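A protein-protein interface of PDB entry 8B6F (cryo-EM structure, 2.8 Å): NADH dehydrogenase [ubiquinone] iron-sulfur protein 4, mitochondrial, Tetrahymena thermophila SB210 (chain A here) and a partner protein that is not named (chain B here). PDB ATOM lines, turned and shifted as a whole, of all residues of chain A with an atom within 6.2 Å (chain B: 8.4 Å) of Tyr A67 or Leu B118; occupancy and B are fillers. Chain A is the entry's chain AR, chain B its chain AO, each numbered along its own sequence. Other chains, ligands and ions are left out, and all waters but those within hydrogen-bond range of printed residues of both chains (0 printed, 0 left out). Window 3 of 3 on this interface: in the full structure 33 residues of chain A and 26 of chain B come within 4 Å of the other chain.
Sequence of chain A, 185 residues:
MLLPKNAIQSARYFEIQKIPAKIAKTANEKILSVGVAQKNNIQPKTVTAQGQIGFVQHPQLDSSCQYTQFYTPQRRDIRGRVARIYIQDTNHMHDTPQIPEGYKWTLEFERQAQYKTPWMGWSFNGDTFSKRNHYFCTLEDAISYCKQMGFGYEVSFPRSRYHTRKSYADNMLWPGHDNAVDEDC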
ATOM      1  N   SER A  63     -24.498 -34.617 -38.787  1.00  0.00           N
ATOM      2  CA  SER A  63     -25.129 -33.529 -38.055  1.00  0.00           C
ATOM      3  C   SER A  63     -24.472 -33.285 -36.705  1.00  0.00           C
ATOM      4  O   SER A  63     -24.714 -32.237 -36.097  1.00  0.00           O
ATOM      5  CB  SER A  63     -26.618 -33.814 -37.857  1.00  0.00           C
ATOM      6  OG  SER A  63     -26.814 -34.986 -37.087  1.00  0.00           O
ATOM      7  N   SER A  64     -23.649 -34.221 -36.226  1.00  0.00           N
ATOM      8  CA  SER A  64     -23.035 -34.080 -34.913  1.00  0.00           C
ATOM      9  C   SER A  64     -21.898 -33.069 -34.916  1.00  0.00           C
ATOM     10  O   SER A  64     -21.592 -32.487 -33.870  1.00  0.00           O
ATOM     11  CB  SER A  64     -22.525 -35.437 -34.425  1.00  0.00           C
ATOM     12  OG  SER A  64     -21.515 -35.940 -35.281  1.00  0.00           O
ATOM     13  N   CYS A  65     -21.259 -32.845 -36.068  1.00  0.00           N
ATOM     14  CA  CYS A  65     -20.131 -31.926 -36.165  1.00  0.00           C
ATOM     15  C   CYS A  65     -20.562 -30.511 -36.527  1.00  0.00           C
ATOM     16  O   CYS A  65     -19.780 -29.758 -37.121  1.00  0.00           O
ATOM     17  CB  CYS A  65     -19.115 -32.448 -37.183  1.00  0.00           C
ATOM     18  SG  CYS A  65     -19.574 -32.183 -38.907  1.00  0.00           S
ATOM     19  N   GLN A  66     -21.791 -30.131 -36.179  1.00  0.00           N
ATOM     20  CA  GLN A  66     -22.297 -28.803 -36.499  1.00  0.00           C
ATOM     21  C   GLN A  66     -21.623 -27.703 -35.688  1.00  0.00           C
ATOM     22  O   GLN A  66     -21.691 -26.534 -36.079  1.00  0.00           O
ATOM     23  CB  GLN A  66     -23.809 -28.758 -36.272  1.00  0.00           C
ATOM     24  CG  GLN A  66     -24.237 -29.166 -34.871  1.00  0.00           C
ATOM     25  CD  GLN A  66     -25.738 -29.228 -34.720  1.00  0.00           C
ATOM     26  OE1 GLN A  66     -26.469 -28.477 -35.360  1.00  0.00           O
ATOM     27  NE2 GLN A  66     -26.209 -30.133 -33.872  1.00  0.00           N
ATOM     28  N   TYR A  67     -20.972 -28.045 -34.579  1.00  0.00           N
ATOM     29  CA  TYR A  67     -20.402 -27.049 -33.682  1.00  0.00           C
ATOM     30  C   TYR A  67     -19.013 -26.586 -34.100  1.00  0.00           C
ATOM     31  O   TYR A  67     -18.447 -25.713 -33.434  1.00  0.00           O
ATOM     32  CB  TYR A  67     -20.350 -27.606 -32.257  1.00  0.00           C
ATOM     33  CG  TYR A  67     -21.688 -28.103 -31.764  1.00  0.00           C
ATOM     34  CD1 TYR A  67     -22.622 -27.227 -31.231  1.00  0.00           C
ATOM     35  CD2 TYR A  67     -22.019 -29.446 -31.839  1.00  0.00           C
ATOM     36  CE1 TYR A  67     -23.848 -27.676 -30.784  1.00  0.00           C
ATOM     37  CE2 TYR A  67     -23.242 -29.907 -31.393  1.00  0.00           C
ATOM     38  CZ  TYR A  67     -24.152 -29.016 -30.866  1.00  0.00           C
ATOM     39  OH  TYR A  67     -25.372 -29.467 -30.421  1.00  0.00           O
ATOM     40  N   THR A  68     -18.452 -27.143 -35.168  1.00  0.00           N
ATOM     41  CA  THR A  68     -17.135 -26.722 -35.622  1.00  0.00           C
ATOM     42  C   THR A  68     -17.179 -25.293 -36.146  1.00  0.00           C
ATOM     43  O   THR A  68     -18.162 -24.867 -36.755  1.00  0.00           O
ATOM     44  CB  THR A  68     -16.625 -27.660 -36.716  1.00  0.00           C
ATOM     45  OG1 THR A  68     -15.279 -27.309 -37.062  1.00  0.00           O
ATOM     46  CG2 THR A  68     -17.503 -27.574 -37.960  1.00  0.00           C
ATOM     47  N   GLN A  69     -16.101 -24.549 -35.902  1.00  0.00           N
ATOM     48  CA  GLN A  69     -15.956 -23.194 -36.410  1.00  0.00           C
ATOM     49  C   GLN A  69     -14.868 -23.074 -37.466  1.00  0.00           C
ATOM     50  O   GLN A  69     -14.679 -21.987 -38.018  1.00  0.00           O
ATOM     51  CB  GLN A  69     -15.655 -22.222 -35.265  1.00  0.00           C
ATOM     52  CG  GLN A  69     -14.404 -22.564 -34.469  1.00  0.00           C
ATOM     53  CD  GLN A  69     -13.817 -21.360 -33.758  1.00  0.00           C
ATOM     54  OE1 GLN A  69     -13.677 -21.353 -32.536  1.00  0.00           O
ATOM     55  NE2 GLN A  69     -13.457 -20.339 -34.524  1.00  0.00           N
ATOM     56  N   SER A 144     -15.260 -36.409 -27.056  1.00  0.00           N
ATOM     57  CA  SER A 144     -16.458 -35.605 -27.259  1.00  0.00           C
ATOM     58  C   SER A 144     -16.140 -34.367 -28.083  1.00  0.00           C
ATOM     59  O   SER A 144     -16.913 -33.984 -28.967  1.00  0.00           O
ATOM     60  CB  SER A 144     -17.060 -35.217 -25.909  1.00  0.00           C
ATOM     61  OG  SER A 144     -18.296 -34.547 -26.078  1.00  0.00           O
ATOM     62  N   GLN A 148     -17.677 -33.465 -31.717  1.00  0.00           N
ATOM     63  CA  GLN A 148     -18.370 -32.196 -31.908  1.00  0.00           C
ATOM     64  C   GLN A 148     -17.760 -31.377 -33.037  1.00  0.00           C
ATOM     65  O   GLN A 148     -18.484 -30.663 -33.738  1.00  0.00           O
ATOM     66  CB  GLN A 148     -18.348 -31.388 -30.612  1.00  0.00           C
ATOM     67  CG  GLN A 148     -19.201 -31.973 -29.506  1.00  0.00           C
ATOM     68  CD  GLN A 148     -18.967 -31.288 -28.177  1.00  0.00           C
ATOM     69  OE1 GLN A 148     -18.219 -30.317 -28.091  1.00  0.00           O
ATOM     70  NE2 GLN A 148     -19.603 -31.797 -27.129  1.00  0.00           N
ATOM     71  N   MET A 149     -16.445 -31.445 -33.219  1.00  0.00           N
ATOM     72  CA  MET A 149     -15.769 -30.658 -34.242  1.00  0.00           C
ATOM     73  C   MET A 149     -15.571 -31.413 -35.550  1.00  0.00           C
ATOM     74  O   MET A 149     -15.037 -30.837 -36.503  1.00  0.00           O
ATOM     75  CB  MET A 149     -14.412 -30.179 -33.718  1.00  0.00           C
ATOM     76  CG  MET A 149     -14.505 -29.394 -32.421  1.00  0.00           C
ATOM     77  SD  MET A 149     -15.640 -27.997 -32.516  1.00  0.00           S
ATOM     78  CE  MET A 149     -15.704 -27.492 -30.800  1.00  0.00           C
ATOM     79  N   ILE B  69     -13.502 -26.305 -20.473  1.00  0.00           N
ATOM     80  CA  ILE B  69     -13.391 -27.667 -20.989  1.00  0.00           C
ATOM     81  C   ILE B  69     -11.939 -28.129 -20.973  1.00  0.00           C
ATOM     82  O   ILE B  69     -11.648 -29.298 -20.697  1.00  0.00           O
ATOM     83  CB  ILE B  69     -14.002 -27.757 -22.402  1.00  0.00           C
ATOM     84  CG1 ILE B  69     -14.199 -29.217 -22.814  1.00  0.00           C
ATOM     85  CG2 ILE B  69     -13.107 -27.086 -23.430  1.00  0.00           C
ATOM     86  CD1 ILE B  69     -15.259 -29.952 -22.018  1.00  0.00           C
ATOM     87  N   LYS B  93     -18.561 -27.276 -20.324  1.00  0.00           N
ATOM     88  CA  LYS B  93     -18.159 -26.681 -21.593  1.00  0.00           C
ATOM     89  C   LYS B  93     -17.739 -25.227 -21.428  1.00  0.00           C
ATOM     90  O   LYS B  93     -16.717 -24.804 -21.980  1.00  0.00           O
ATOM     91  CB  LYS B  93     -19.292 -26.791 -22.613  1.00  0.00           C
ATOM     92  CG  LYS B  93     -18.873 -26.361 -24.009  1.00  0.00           C
ATOM     93  CD  LYS B  93     -19.882 -26.765 -25.071  1.00  0.00           C
ATOM     94  CE  LYS B  93     -19.310 -26.534 -26.464  1.00  0.00           C
ATOM     95  NZ  LYS B  93     -20.264 -26.907 -27.542  1.00  0.00           N
ATOM     96  N   MET B  94     -18.507 -24.444 -20.673  1.00  0.00           N
ATOM     97  CA  MET B  94     -18.200 -23.032 -20.517  1.00  0.00           C
ATOM     98  C   MET B  94     -18.606 -22.577 -19.126  1.00  0.00           C
ATOM     99  O   MET B  94     -19.442 -23.197 -18.466  1.00  0.00           O
ATOM    100  CB  MET B  94     -18.921 -22.194 -21.583  1.00  0.00           C
ATOM    101  CG  MET B  94     -18.394 -20.779 -21.751  1.00  0.00           C
ATOM    102  SD  MET B  94     -16.714 -20.716 -22.399  1.00  0.00           S
ATOM    103  CE  MET B  94     -16.937 -21.437 -24.022  1.00  0.00           C
ATOM    104  N   LEU B 115     -22.312 -23.394 -18.160  1.00  0.00           N
ATOM    105  CA  LEU B 115     -23.027 -23.709 -19.390  1.00  0.00           C
ATOM    106  C   LEU B 115     -22.549 -25.076 -19.862  1.00  0.00           C
ATOM    107  O   LEU B 115     -21.388 -25.231 -20.251  1.00  0.00           O
ATOM    108  CB  LEU B 115     -22.795 -22.641 -20.457  1.00  0.00           C
ATOM    109  CG  LEU B 115     -23.114 -21.204 -20.042  1.00  0.00           C
ATOM    110  CD1 LEU B 115     -22.739 -20.234 -21.145  1.00  0.00           C
ATOM    111  CD2 LEU B 115     -24.583 -21.063 -19.683  1.00  0.00           C
ATOM    112  N   ASN B 116     -23.445 -26.060 -19.823  1.00  0.00           N
ATOM    113  CA  ASN B 116     -23.138 -27.410 -20.268  1.00  0.00           C
ATOM    114  C   ASN B 116     -23.752 -27.755 -21.614  1.00  0.00           C
ATOM    115  O   ASN B 116     -23.254 -28.663 -22.287  1.00  0.00           O
ATOM    116  CB  ASN B 116     -23.606 -28.433 -19.223  1.00  0.00           C
ATOM    117  CG  ASN B 116     -25.067 -28.265 -18.858  1.00  0.00           C
ATOM    118  OD1 ASN B 116     -25.850 -27.702 -19.623  1.00  0.00           O
ATOM    119  ND2 ASN B 116     -25.439 -28.744 -17.676  1.00  0.00           N
ATOM    120  N   ASN B 117     -24.817 -27.067 -22.019  1.00  0.00           N
ATOM    121  CA  ASN B 117     -25.383 -27.286 -23.341  1.00  0.00           C
ATOM    122  C   ASN B 117     -24.379 -26.886 -24.412  1.00  0.00           C
ATOM    123  O   ASN B 117     -23.612 -25.933 -24.247  1.00  0.00           O
ATOM    124  CB  ASN B 117     -26.682 -26.494 -23.503  1.00  0.00           C
ATOM    125  CG  ASN B 117     -26.531 -25.037 -23.110  1.00  0.00           C
ATOM    126  OD1 ASN B 117     -25.420 -24.525 -22.989  1.00  0.00           O
ATOM    127  ND2 ASN B 117     -27.655 -24.361 -22.906  1.00  0.00           N
ATOM    128  N   LEU B 118     -24.384 -27.626 -25.519  1.00  0.00           N
ATOM    129  CA  LEU B 118     -23.371 -27.431 -26.550  1.00  0.00           C
ATOM    130  C   LEU B 118     -23.498 -26.074 -27.231  1.00  0.00           C
ATOM    131  O   LEU B 118     -22.491 -25.510 -27.671  1.00  0.00           O
ATOM    132  CB  LEU B 118     -23.462 -28.554 -27.581  1.00  0.00           C
ATOM    133  CG  LEU B 118     -23.393 -29.975 -27.013  1.00  0.00           C
ATOM    134  CD1 LEU B 118     -23.467 -31.000 -28.129  1.00  0.00           C
ATOM    135  CD2 LEU B 118     -22.133 -30.176 -26.187  1.00  0.00           C
ATOM    136  N   ASN B 119     -24.712 -25.537 -27.332  1.00  0.00           N
ATOM    137  CA  ASN B 119     -24.921 -24.269 -28.021  1.00  0.00           C
ATOM    138  C   ASN B 119     -24.668 -23.058 -27.131  1.00  0.00           C
ATOM    139  O   ASN B 119     -24.683 -21.930 -27.637  1.00  0.00           O
ATOM    140  CB  ASN B 119     -26.341 -24.207 -28.591  1.00  0.00           C
ATOM    141  CG  ASN B 119     -27.405 -24.454 -27.545  1.00  0.00           C
ATOM    142  OD1 ASN B 119     -27.229 -24.131 -26.372  1.00  0.00           O
ATOM    143  ND2 ASN B 119     -28.520 -25.039 -27.966  1.00  0.00           N
ATOM    144  N   LYS B 120     -24.436 -23.254 -25.833  1.00  0.00           N
ATOM    145  CA  LYS B 120     -24.072 -22.168 -24.926  1.00  0.00           C
ATOM    146  C   LYS B 120     -25.181 -21.116 -24.847  1.00  0.00           C
ATOM    147  O   LYS B 120     -24.975 -19.932 -25.113  1.00  0.00           O
ATOM    148  CB  LYS B 120     -22.748 -21.530 -25.355  1.00  0.00           C
ATOM    149  CG  LYS B 120     -21.614 -22.516 -25.579  1.00  0.00           C
ATOM    150  CD  LYS B 120     -20.414 -21.820 -26.202  1.00  0.00           C
ATOM    151  CE  LYS B 120     -19.354 -22.813 -26.637  1.00  0.00           C
ATOM    152  NZ  LYS B 120     -18.228 -22.146 -27.344  1.00  0.00           N
ATOM    153  N   ASN B 121     -26.371 -21.573 -24.468  1.00  0.00           N
ATOM    154  CA  ASN B 121     -27.525 -20.697 -24.331  1.00  0.00           C
ATOM    155  C   ASN B 121     -27.611 -20.145 -22.914  1.00  0.00           C
ATOM    156  O   ASN B 121     -27.433 -20.876 -21.937  1.00  0.00           O
ATOM    157  CB  ASN B 121     -28.818 -21.444 -24.667  1.00  0.00           C
ATOM    158  CG  ASN B 121     -29.021 -21.612 -26.157  1.00  0.00           C
ATOM    159  OD1 ASN B 121     -28.551 -20.804 -26.955  1.00  0.00           O
ATOM    160  ND2 ASN B 121     -29.733 -22.665 -26.540  1.00  0.00           N
ATOM    161  N   TYR B 143     -16.278 -15.920 -27.374  1.00  0.00           N
ATOM    162  CA  TYR B 143     -16.432 -17.279 -26.882  1.00  0.00           C
ATOM    163  C   TYR B 143     -17.616 -18.019 -27.487  1.00  0.00           C
ATOM    164  O   TYR B 143     -17.756 -19.222 -27.241  1.00  0.00           O
ATOM    165  CB  TYR B 143     -16.577 -17.279 -25.352  1.00  0.00           C
ATOM    166  CG  TYR B 143     -15.305 -16.918 -24.625  1.00  0.00           C
ATOM    167  CD1 TYR B 143     -14.372 -17.891 -24.290  1.00  0.00           C
ATOM    168  CD2 TYR B 143     -15.037 -15.604 -24.269  1.00  0.00           C
ATOM    169  CE1 TYR B 143     -13.207 -17.564 -23.625  1.00  0.00           C
ATOM    170  CE2 TYR B 143     -13.878 -15.267 -23.604  1.00  0.00           C
ATOM    171  CZ  TYR B 143     -12.966 -16.250 -23.285  1.00  0.00           C
ATOM    172  OH  TYR B 143     -11.809 -15.915 -22.624  1.00  0.00           O
ATOM    173  N   GLY B 144     -18.463 -17.351 -28.263  1.00  0.00           N
ATOM    174  CA  GLY B 144     -19.566 -18.026 -28.915  1.00  0.00           C
ATOM    175  C   GLY B 144     -20.761 -18.308 -28.036  1.00  0.00           C
ATOM    176  O   GLY B 144     -21.520 -19.235 -28.328  1.00  0.00           O
ATOM    177  N   ILE B 145     -20.955 -17.541 -26.964  1.00  0.00           N
ATOM    178  CA  ILE B 145     -22.126 -17.724 -26.116  1.00  0.00           C
ATOM    179  C   ILE B 145     -23.352 -17.169 -26.827  1.00  0.00           C
ATOM    180  O   ILE B 145     -23.338 -16.040 -27.333  1.00  0.00           O
ATOM    181  CB  ILE B 145     -21.919 -17.053 -24.748  1.00  0.00           C
ATOM    182  CG1 ILE B 145     -21.008 -17.899 -23.854  1.00  0.00           C
ATOM    183  CG2 ILE B 145     -23.249 -16.827 -24.034  1.00  0.00           C
ATOM    184  CD1 ILE B 145     -19.575 -17.967 -24.307  1.00  0.00           C
ATOM    185  N   ASN B 146     -24.419 -17.963 -26.870  1.00  0.00           N
ATOM    186  CA  ASN B 146     -25.663 -17.566 -27.525  1.00  0.00           C
ATOM    187  C   ASN B 146     -26.546 -16.882 -26.491  1.00  0.00           C
ATOM    188  O   ASN B 146     -27.400 -17.505 -25.860  1.00  0.00           O
ATOM    189  CB  ASN B 146     -26.354 -18.773 -28.144  1.00  0.00           C
ATOM    190  CG  ASN B 146     -27.719 -18.436 -28.708  1.00  0.00           C
ATOM    191  OD1 ASN B 146     -28.000 -17.286 -29.040  1.00  0.00           O
ATOM    192  ND2 ASN B 146     -28.578 -19.441 -28.818  1.00  0.00           N
ATOM    193  N   ASN B 165     -14.591 -17.401 -33.100  1.00  0.00           N
ATOM    194  CA  ASN B 165     -14.561 -17.216 -31.650  1.00  0.00           C
ATOM    195  C   ASN B 165     -13.116 -17.389 -31.204  1.00  0.00           C
ATOM    196  O   ASN B 165     -12.729 -18.453 -30.703  1.00  0.00           O
ATOM    197  CB  ASN B 165     -15.492 -18.203 -30.947  1.00  0.00           C
ATOM    198  CG  ASN B 165     -16.894 -18.187 -31.519  1.00  0.00           C
ATOM    199  OD1 ASN B 165     -17.445 -19.229 -31.870  1.00  0.00           O
ATOM    200  ND2 ASN B 165     -17.478 -17.000 -31.620  1.00  0.00           N
ATOM    201  N   LEU B 168     -11.610 -19.047 -27.733  1.00  0.00           N
ATOM    202  CA  LEU B 168     -11.686 -20.468 -27.425  1.00  0.00           C
ATOM    203  C   LEU B 168     -10.301 -21.094 -27.504  1.00  0.00           C
ATOM    204  O   LEU B 168      -9.495 -20.752 -28.372  1.00  0.00           O
ATOM    205  CB  LEU B 168     -12.641 -21.170 -28.389  1.00  0.00           C
ATOM    206  CG  LEU B 168     -14.116 -20.770 -28.293  1.00  0.00           C
ATOM    207  CD1 LEU B 168     -14.926 -21.465 -29.371  1.00  0.00           C
ATOM    208  CD2 LEU B 168     -14.679 -21.090 -26.918  1.00  0.00           C
ATOM    209  N   GLU B 170      -9.371 -23.832 -28.566  1.00  0.00           N
ATOM    210  CA  GLU B 170      -9.098 -24.522 -29.822  1.00  0.00           C
ATOM    211  C   GLU B 170      -8.446 -23.587 -30.833  1.00  0.00           C
ATOM    212  O   GLU B 170      -7.595 -24.011 -31.621  1.00  0.00           O
ATOM    213  CB  GLU B 170     -10.389 -25.106 -30.393  1.00  0.00           C
ATOM    214  CG  GLU B 170     -11.446 -24.062 -30.724  1.00  0.00           C
ATOM    215  CD  GLU B 170     -12.704 -24.674 -31.297  1.00  0.00           C
ATOM    216  OE1 GLU B 170     -12.761 -25.915 -31.415  1.00  0.00           O
ATOM    217  OE2 GLU B 170     -13.638 -23.916 -31.632  1.00  0.00           O
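The backbone NH (N) of Asn B165 sits close to the side-chain amide nitrogen (NE2) of Gln A69, at 3.5 Å. The side-chain carboxylate of Glu B170 sits close to the side-chain amide oxygen of Gln A69, at 2.7 Å. OE1 of Glu B170 sits close to SD of Met A149 (3.7 Å).
The backbone carbonyl oxygen (O) of Leu B118 sits at hydrogen-bond distance from the side-chain amino group (NZ) of Lys B93 (2.6 Å). The side-chain amide nitrogen of Gln A148 is in hydrogen-bond range of the side-chain hydroxyl of Ser A144 (3.2 Å).
Among the printed residues, pairs that only touch across the chains: Gln A148 with Leu B118 (3.1 Å), Tyr A67 with Leu B118 (3.3 Å) and Gln A69 with Leu B168 (3.4 Å).
Of chain B, only Leu B118 comes within 4 Å of Tyr A67. Leu B118 touches two residues of chain A. Printed residues of chain B within 4 Å of Gln A69: Asn B165, Leu B168 and Glu B170. Of the printed residues of chain A, Glu B170 touches Gln A69 and Met A149. Of the printed residues of chain A, Leu B168 touches Gln A69. Ile B69 touches none of the printed residues of chain A. The nearest residue of chain B that does not touch Tyr A67 is Asn B119 (4.2 Å). The nearest residue of chain A that does not touch Leu B118 is Ser A144 (5.8 Å). The nearest printed residue of chain A that does not touch Leu B168 is Met A149 (6.2 Å).
Of the 10 printed residues of chain A, 4 touch a printed residue of chain B. Hydrophobic or aromatic side chains of chain A within 4 Å of the printed part of chain B: Tyr A67 and Met A149. Hydrophobic or aromatic side chains of chain B that line the printed part of chain A: Leu B118 and Leu B168. Among the printed residues, 6 pairs touch across the chains. Among the printed residues, no Asp or Glu carboxylate lies within 4 Å of a Lys or Arg side-chain nitrogen of the other chain.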
